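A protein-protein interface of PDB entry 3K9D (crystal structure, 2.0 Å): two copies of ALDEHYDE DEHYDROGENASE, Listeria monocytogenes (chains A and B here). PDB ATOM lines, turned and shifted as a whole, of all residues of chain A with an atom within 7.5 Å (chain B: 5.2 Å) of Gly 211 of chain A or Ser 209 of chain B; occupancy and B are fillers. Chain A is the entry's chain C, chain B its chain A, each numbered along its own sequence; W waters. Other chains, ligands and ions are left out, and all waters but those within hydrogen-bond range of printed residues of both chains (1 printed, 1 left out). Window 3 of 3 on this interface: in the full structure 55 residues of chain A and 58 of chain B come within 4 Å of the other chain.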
ATOM      1  N   MET A 187      34.572 -20.969  23.688  1.00  0.00           N
ATOM      2  CA  MET A 187      33.154 -20.714  23.829  1.00  0.00           C
ATOM      3  C   MET A 187      32.887 -19.532  24.767  1.00  0.00           C
ATOM      4  O   MET A 187      32.147 -18.618  24.407  1.00  0.00           O
ATOM      5  CB  MET A 187      32.414 -21.984  24.293  1.00  0.00           C
ATOM      6  CG  MET A 187      32.353 -23.124  23.213  1.00  0.00           C
ATOM      7  SD  MET A 187      31.130 -24.463  23.411  1.00  0.00           S
ATOM      8  CE  MET A 187      31.455 -25.013  25.076  1.00  0.00           C
ATOM      9  N   LYS A 188      33.508 -19.540  25.947  1.00  0.00           N
ATOM     10  CA  LYS A 188      33.210 -18.560  26.998  1.00  0.00           C
ATOM     11  C   LYS A 188      33.817 -17.168  26.776  1.00  0.00           C
ATOM     12  O   LYS A 188      33.413 -16.210  27.446  1.00  0.00           O
ATOM     13  CB  LYS A 188      33.672 -19.068  28.366  1.00  0.00           C
ATOM     14  CG  LYS A 188      32.813 -20.142  29.004  1.00  0.00           C
ATOM     15  CD  LYS A 188      33.166 -20.266  30.489  1.00  0.00           C
ATOM     16  CE  LYS A 188      32.789 -21.619  31.086  1.00  0.00           C
ATOM     17  NZ  LYS A 188      31.355 -21.948  30.953  1.00  0.00           N
ATOM     18  N   HIS A 189      34.777 -17.063  25.855  1.00  0.00           N
ATOM     19  CA  HIS A 189      35.604 -15.860  25.716  1.00  0.00           C
ATOM     20  C   HIS A 189      34.791 -14.635  25.346  1.00  0.00           C
ATOM     21  O   HIS A 189      33.946 -14.698  24.462  1.00  0.00           O
ATOM     22  CB  HIS A 189      36.682 -16.057  24.663  1.00  0.00           C
ATOM     23  CG  HIS A 189      37.897 -15.205  24.875  1.00  0.00           C
ATOM     24  ND1 HIS A 189      37.913 -13.849  24.624  1.00  0.00           N
ATOM     25  CD2 HIS A 189      39.140 -15.520  25.312  1.00  0.00           C
ATOM     26  CE1 HIS A 189      39.112 -13.365  24.897  1.00  0.00           C
ATOM     27  NE2 HIS A 189      39.875 -14.356  25.320  1.00  0.00           N
ATOM     28  N   THR A 192      34.680 -13.786  21.743  1.00  0.00           N
ATOM     29  CA  THR A 192      34.004 -14.708  20.859  1.00  0.00           C
ATOM     30  C   THR A 192      32.577 -14.186  20.744  1.00  0.00           C
ATOM     31  O   THR A 192      31.884 -14.014  21.754  1.00  0.00           O
ATOM     32  CB  THR A 192      34.093 -16.163  21.381  1.00  0.00           C
ATOM     33  OG1 THR A 192      35.468 -16.605  21.344  1.00  0.00           O
ATOM     34  CG2 THR A 192      33.217 -17.112  20.551  1.00  0.00           C
ATOM     35  N   ALA A 193      32.166 -13.923  19.505  1.00  0.00           N
ATOM     36  CA  ALA A 193      30.877 -13.311  19.197  1.00  0.00           C
ATOM     37  C   ALA A 193      29.728 -14.315  19.108  1.00  0.00           C
ATOM     38  O   ALA A 193      28.637 -14.083  19.659  1.00  0.00           O
ATOM     39  CB  ALA A 193      30.986 -12.529  17.918  1.00  0.00           C
ATOM     40  N   ILE A 195      28.948 -18.887  18.694  1.00  0.00           N
ATOM     41  CA  ILE A 195      29.399 -20.268  18.543  1.00  0.00           C
ATOM     42  C   ILE A 195      28.529 -20.972  17.510  1.00  0.00           C
ATOM     43  O   ILE A 195      27.315 -21.051  17.684  1.00  0.00           O
ATOM     44  CB  ILE A 195      29.312 -21.041  19.871  1.00  0.00           C
ATOM     45  CG1 ILE A 195      30.061 -20.287  20.981  1.00  0.00           C
ATOM     46  CG2 ILE A 195      29.842 -22.483  19.700  1.00  0.00           C
ATOM     47  CD1 ILE A 195      29.617 -20.663  22.373  1.00  0.00           C
ATOM     48  N   LYS A 205      24.252 -27.987  24.470  1.00  0.00           N
ATOM     49  CA  LYS A 205      23.861 -27.496  25.800  1.00  0.00           C
ATOM     50  C   LYS A 205      24.963 -26.669  26.489  1.00  0.00           C
ATOM     51  O   LYS A 205      24.662 -25.678  27.163  1.00  0.00           O
ATOM     52  CB  LYS A 205      23.426 -28.653  26.708  1.00  0.00           C
ATOM     53  CG  LYS A 205      22.690 -28.236  27.988  1.00  0.00           C
ATOM     54  CD  LYS A 205      22.446 -29.430  28.925  1.00  0.00           C
ATOM     55  CE  LYS A 205      21.189 -30.231  28.540  1.00  0.00           C
ATOM     56  NZ  LYS A 205      20.880 -31.352  29.492  1.00  0.00           N
ATOM     57  N   ALA A 206      26.222 -27.079  26.307  1.00  0.00           N
ATOM     58  CA  ALA A 206      27.371 -26.314  26.786  1.00  0.00           C
ATOM     59  C   ALA A 206      27.454 -24.945  26.109  1.00  0.00           C
ATOM     60  O   ALA A 206      27.649 -23.930  26.781  1.00  0.00           O
ATOM     61  CB  ALA A 206      28.674 -27.099  26.584  1.00  0.00           C
ATOM     62  N   ALA A 207      27.272 -24.926  24.790  1.00  0.00           N
ATOM     63  CA  ALA A 207      27.319 -23.697  24.012  1.00  0.00           C
ATOM     64  C   ALA A 207      26.231 -22.690  24.400  1.00  0.00           C
ATOM     65  O   ALA A 207      26.462 -21.477  24.333  1.00  0.00           O
ATOM     66  CB  ALA A 207      27.269 -24.001  22.521  1.00  0.00           C
ATOM     67  N   TYR A 208      25.063 -23.190  24.812  1.00  0.00           N
ATOM     68  CA  TYR A 208      23.960 -22.334  25.274  1.00  0.00           C
ATOM     69  C   TYR A 208      24.077 -21.982  26.743  1.00  0.00           C
ATOM     70  O   TYR A 208      23.292 -21.182  27.253  1.00  0.00           O
ATOM     71  CB  TYR A 208      22.580 -22.941  24.928  1.00  0.00           C
ATOM     72  CG  TYR A 208      22.213 -22.720  23.475  1.00  0.00           C
ATOM     73  CD1 TYR A 208      21.661 -21.509  23.050  1.00  0.00           C
ATOM     74  CD2 TYR A 208      22.487 -23.692  22.513  1.00  0.00           C
ATOM     75  CE1 TYR A 208      21.364 -21.284  21.715  1.00  0.00           C
ATOM     76  CE2 TYR A 208      22.192 -23.479  21.171  1.00  0.00           C
ATOM     77  CZ  TYR A 208      21.626 -22.272  20.781  1.00  0.00           C
ATOM     78  OH  TYR A 208      21.332 -22.061  19.456  1.00  0.00           O
ATOM     79  N   SER A 209      25.072 -22.575  27.410  1.00  0.00           N
ATOM     80  CA  SER A 209      25.377 -22.270  28.808  1.00  0.00           C
ATOM     81  C   SER A 209      26.687 -21.503  28.964  1.00  0.00           C
ATOM     82  O   SER A 209      27.171 -21.322  30.080  1.00  0.00           O
ATOM     83  CB  SER A 209      25.420 -23.552  29.653  1.00  0.00           C
ATOM     84  OG  SER A 209      24.294 -24.383  29.393  1.00  0.00           O
ATOM     85  N   SER A 210      27.247 -21.045  27.848  1.00  0.00           N
ATOM     86  CA  SER A 210      28.597 -20.454  27.816  1.00  0.00           C
ATOM     87  C   SER A 210      28.663 -18.961  28.144  1.00  0.00           C
ATOM     88  O   SER A 210      29.727 -18.457  28.533  1.00  0.00           O
ATOM     89  CB  SER A 210      29.203 -20.654  26.437  1.00  0.00           C
ATOM     90  OG  SER A 210      28.528 -19.847  25.493  1.00  0.00           O
ATOM     91  N   GLY A 211      27.542 -18.263  27.947  1.00  0.00           N
ATOM     92  CA  GLY A 211      27.492 -16.801  28.058  1.00  0.00           C
ATOM     93  C   GLY A 211      27.568 -16.107  26.707  1.00  0.00           C
ATOM     94  O   GLY A 211      27.354 -14.901  26.606  1.00  0.00           O
ATOM     95  N   THR A 212      27.880 -16.877  25.670  1.00  0.00           N
ATOM     96  CA  THR A 212      28.110 -16.359  24.328  1.00  0.00           C
ATOM     97  C   THR A 212      26.908 -16.826  23.555  1.00  0.00           C
ATOM     98  O   THR A 212      26.438 -17.947  23.801  1.00  0.00           O
ATOM     99  CB  THR A 212      29.428 -16.944  23.721  1.00  0.00           C
ATOM    100  OG1 THR A 212      30.544 -16.539  24.515  1.00  0.00           O
ATOM    101  CG2 THR A 212      29.691 -16.486  22.285  1.00  0.00           C
ATOM    102  N   PRO A 213      26.359 -15.963  22.669  1.00  0.00           N
ATOM    103  CA  PRO A 213      25.292 -16.415  21.783  1.00  0.00           C
ATOM    104  C   PRO A 213      25.742 -17.628  20.977  1.00  0.00           C
ATOM    105  O   PRO A 213      26.866 -17.662  20.467  1.00  0.00           O
ATOM    106  CB  PRO A 213      25.058 -15.208  20.867  1.00  0.00           C
ATOM    107  CG  PRO A 213      25.445 -14.029  21.708  1.00  0.00           C
ATOM    108  CD  PRO A 213      26.651 -14.530  22.477  1.00  0.00           C
ATOM    109  N   ALA A 214      24.870 -18.623  20.900  1.00  0.00           N
ATOM    110  CA  ALA A 214      25.185 -19.880  20.239  1.00  0.00           C
ATOM    111  C   ALA A 214      24.145 -20.159  19.179  1.00  0.00           C
ATOM    112  O   ALA A 214      22.975 -19.756  19.304  1.00  0.00           O
ATOM    113  CB  ALA A 214      25.199 -21.006  21.247  1.00  0.00           C
ATOM    114  N   LYS B 188      16.293 -21.637  33.097  1.00  0.00           N
ATOM    115  CA  LYS B 188      16.956 -22.953  32.869  1.00  0.00           C
ATOM    116  C   LYS B 188      16.037 -24.096  32.434  1.00  0.00           C
ATOM    117  O   LYS B 188      16.502 -25.060  31.818  1.00  0.00           O
ATOM    118  CB  LYS B 188      17.778 -23.395  34.091  1.00  0.00           C
ATOM    119  CG  LYS B 188      19.118 -22.659  34.251  1.00  0.00           C
ATOM    120  CD  LYS B 188      19.903 -23.146  35.468  1.00  0.00           C
ATOM    121  CE  LYS B 188      21.240 -22.410  35.633  1.00  0.00           C
ATOM    122  NZ  LYS B 188      22.320 -22.886  34.715  1.00  0.00           N
ATOM    123  N   LYS B 205      23.685 -11.679  30.895  1.00  0.00           N
ATOM    124  CA  LYS B 205      24.764 -12.665  30.912  1.00  0.00           C
ATOM    125  C   LYS B 205      24.297 -13.959  31.570  1.00  0.00           C
ATOM    126  O   LYS B 205      24.762 -15.040  31.189  1.00  0.00           O
ATOM    127  CB  LYS B 205      26.038 -12.123  31.571  1.00  0.00           C
ATOM    128  CG  LYS B 205      27.300 -12.931  31.211  1.00  0.00           C
ATOM    129  CD  LYS B 205      28.589 -12.282  31.709  1.00  0.00           C
ATOM    130  CE  LYS B 205      29.088 -11.189  30.758  1.00  0.00           C
ATOM    131  NZ  LYS B 205      30.567 -10.984  30.865  1.00  0.00           N
ATOM    132  N   ALA B 206      23.346 -13.853  32.514  1.00  0.00           N
ATOM    133  CA  ALA B 206      22.715 -15.021  33.141  1.00  0.00           C
ATOM    134  C   ALA B 206      21.866 -15.807  32.151  1.00  0.00           C
ATOM    135  O   ALA B 206      21.835 -17.037  32.204  1.00  0.00           O
ATOM    136  CB  ALA B 206      21.864 -14.619  34.358  1.00  0.00           C
ATOM    137  N   ALA B 207      21.181 -15.081  31.267  1.00  0.00           N
ATOM    138  CA  ALA B 207      20.293 -15.664  30.263  1.00  0.00           C
ATOM    139  C   ALA B 207      21.079 -16.459  29.218  1.00  0.00           C
ATOM    140  O   ALA B 207      20.647 -17.528  28.775  1.00  0.00           O
ATOM    141  CB  ALA B 207      19.470 -14.576  29.591  1.00  0.00           C
ATOM    142  N   TYR B 208      22.243 -15.943  28.834  1.00  0.00           N
ATOM    143  CA  TYR B 208      23.087 -16.650  27.872  1.00  0.00           C
ATOM    144  C   TYR B 208      23.920 -17.770  28.494  1.00  0.00           C
ATOM    145  O   TYR B 208      24.618 -18.509  27.783  1.00  0.00           O
ATOM    146  CB  TYR B 208      23.957 -15.673  27.076  1.00  0.00           C
ATOM    147  CG  TYR B 208      23.185 -14.980  25.984  1.00  0.00           C
ATOM    148  CD1 TYR B 208      22.881 -15.636  24.786  1.00  0.00           C
ATOM    149  CD2 TYR B 208      22.737 -13.667  26.157  1.00  0.00           C
ATOM    150  CE1 TYR B 208      22.158 -14.989  23.775  1.00  0.00           C
ATOM    151  CE2 TYR B 208      22.012 -13.015  25.168  1.00  0.00           C
ATOM    152  CZ  TYR B 208      21.728 -13.672  23.983  1.00  0.00           C
ATOM    153  OH  TYR B 208      21.005 -13.005  23.020  1.00  0.00           O
ATOM    154  N   SER B 209      23.820 -17.907  29.817  1.00  0.00           N
ATOM    155  CA  SER B 209      24.466 -18.987  30.551  1.00  0.00           C
ATOM    156  C   SER B 209      23.472 -20.046  31.055  1.00  0.00           C
ATOM    157  O   SER B 209      23.862 -20.984  31.749  1.00  0.00           O
ATOM    158  CB  SER B 209      25.263 -18.408  31.716  1.00  0.00           C
ATOM    159  OG  SER B 209      26.140 -17.395  31.245  1.00  0.00           O
ATOM    160  N   SER B 210      22.207 -19.898  30.671  1.00  0.00           N
ATOM    161  CA  SER B 210      21.093 -20.708  31.188  1.00  0.00           C
ATOM    162  C   SER B 210      20.917 -22.093  30.540  1.00  0.00           C
ATOM    163  O   SER B 210      20.260 -22.981  31.117  1.00  0.00           O
ATOM    164  CB  SER B 210      19.788 -19.930  31.029  1.00  0.00           C
ATOM    165  OG  SER B 210      19.471 -19.744  29.656  1.00  0.00           O
ATOM    166  N   GLY B 211      21.479 -22.269  29.343  1.00  0.00           N
ATOM    167  CA  GLY B 211      21.223 -23.470  28.547  1.00  0.00           C
ATOM    168  C   GLY B 211      20.033 -23.335  27.615  1.00  0.00           C
ATOM    169  O   GLY B 211      19.784 -24.214  26.799  1.00  0.00           O
ATOM    170  N   GLY B 427      26.936  -8.536  22.933  1.00  0.00           N
ATOM    171  CA  GLY B 427      26.767  -9.866  23.532  1.00  0.00           C
ATOM    172  C   GLY B 427      25.403 -10.524  23.394  1.00  0.00           C
ATOM    173  O   GLY B 427      25.055 -11.424  24.177  1.00  0.00           O
HETATM  174  O   HOH W   1      26.147 -12.499  26.196  1.00  0.00           O
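Tyr 208 of chain A touches its own counterpart, Tyr 208 of chain B.
Tyr 208 of chain A touches Ser 209 of chain B, and with the chains exchanged Ser 209 of chain A touches Tyr 208 of chain B.
Ser 209 of chain B touches its own counterpart, Ser 209 of chain A.
Ser 209 of chain A touches Gly 211 of chain B, and with the chains exchanged Gly 211 of chain A touches Ser 209 of chain B.
Of the 12 pairs that touch across the chains among the printed residues, 10 have their exchanged pair printed and touching as well.
Water W1 lies within hydrogen-bond range of the backbone carbonyl oxygen (O) of Gly 427 of chain B (2.5 Å) and the backbone carbonyl oxygen (O) of Gly 211 of chain A (2.7 Å).
Among the printed residues, merely in contact across the chains: Ser 209 of chain A with Gly 211 of chain B, Gly 211 of chain A with Ser 209 of chain B, Ser 209 of chain A with Ser 209 of chain B, Pro 213 of chain A with Gly 427 of chain B, Ser 210 of chain A with Tyr 208 of chain B, Tyr 208 of chain A with Ser 210 of chain B, Ser 209 of chain A with Tyr 208 of chain B, Pro 213 of chain A with Tyr 208 of chain B and Tyr 208 of chain A with Ser 209 of chain B.
O of Tyr 208 of chain B is in hydrogen-bond range of N of Gly 211 of chain A (2.9 Å).
O of Tyr 208 of chain A is in hydrogen-bond range of N of Gly 211 of chain B, at 3.0 Å.
O of Tyr 208 of chain A lies close to O of Tyr 208 of chain B (3.0 Å).
Gly 211 of chain A touches two residues of chain B.
Ser 209 of chain B touches just these residues of chain A: Tyr 208, Ser 209 and Gly 211.
Printed residues of chain B within 4 Å of Ser 209 of chain A: Tyr 208, Ser 209 and Gly 211.
Printed residues of chain B within 4 Å of Ser 210 of chain A: Tyr 208 (3.7 Å).
Of the printed residues of chain B, Pro 213 of chain A touches Tyr 208 (3.9 Å) and Gly 427 (3.6 Å).
Lys 188 of chain A touches none of the printed residues of chain B.
OG of Ser 209 of chain B lies within hydrogen-bond range of O of Lys 205 of chain B, 2.7 Å away.
O of Ala 207 of chain B lies within hydrogen-bond range of OG of Ser 210 of chain B, at 2.7 Å.
The backbone NH of Ile 195 of chain A lies within hydrogen-bond range of the backbone carbonyl oxygen of Pro 213 of chain A (3.0 Å).
The backbone carbonyl oxygen of Lys 205 of chain A is in hydrogen-bond range of the side-chain hydroxyl of Ser 209 of chain A, at 2.6 Å.
The backbone carbonyl oxygen (O) of Ala 207 of chain A sits at hydrogen-bond distance from the side-chain hydroxyl (OG) of Ser 210 of chain A (2.9 Å).
The side-chain hydroxyl (OG) of Ser 210 of chain A sits at hydrogen-bond distance from the backbone NH (N) of Thr 212 of chain A.
Of the 16 printed residues of chain A, 5 touch a printed residue of chain B.
Among the printed residues, 12 pairs touch across the chains.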
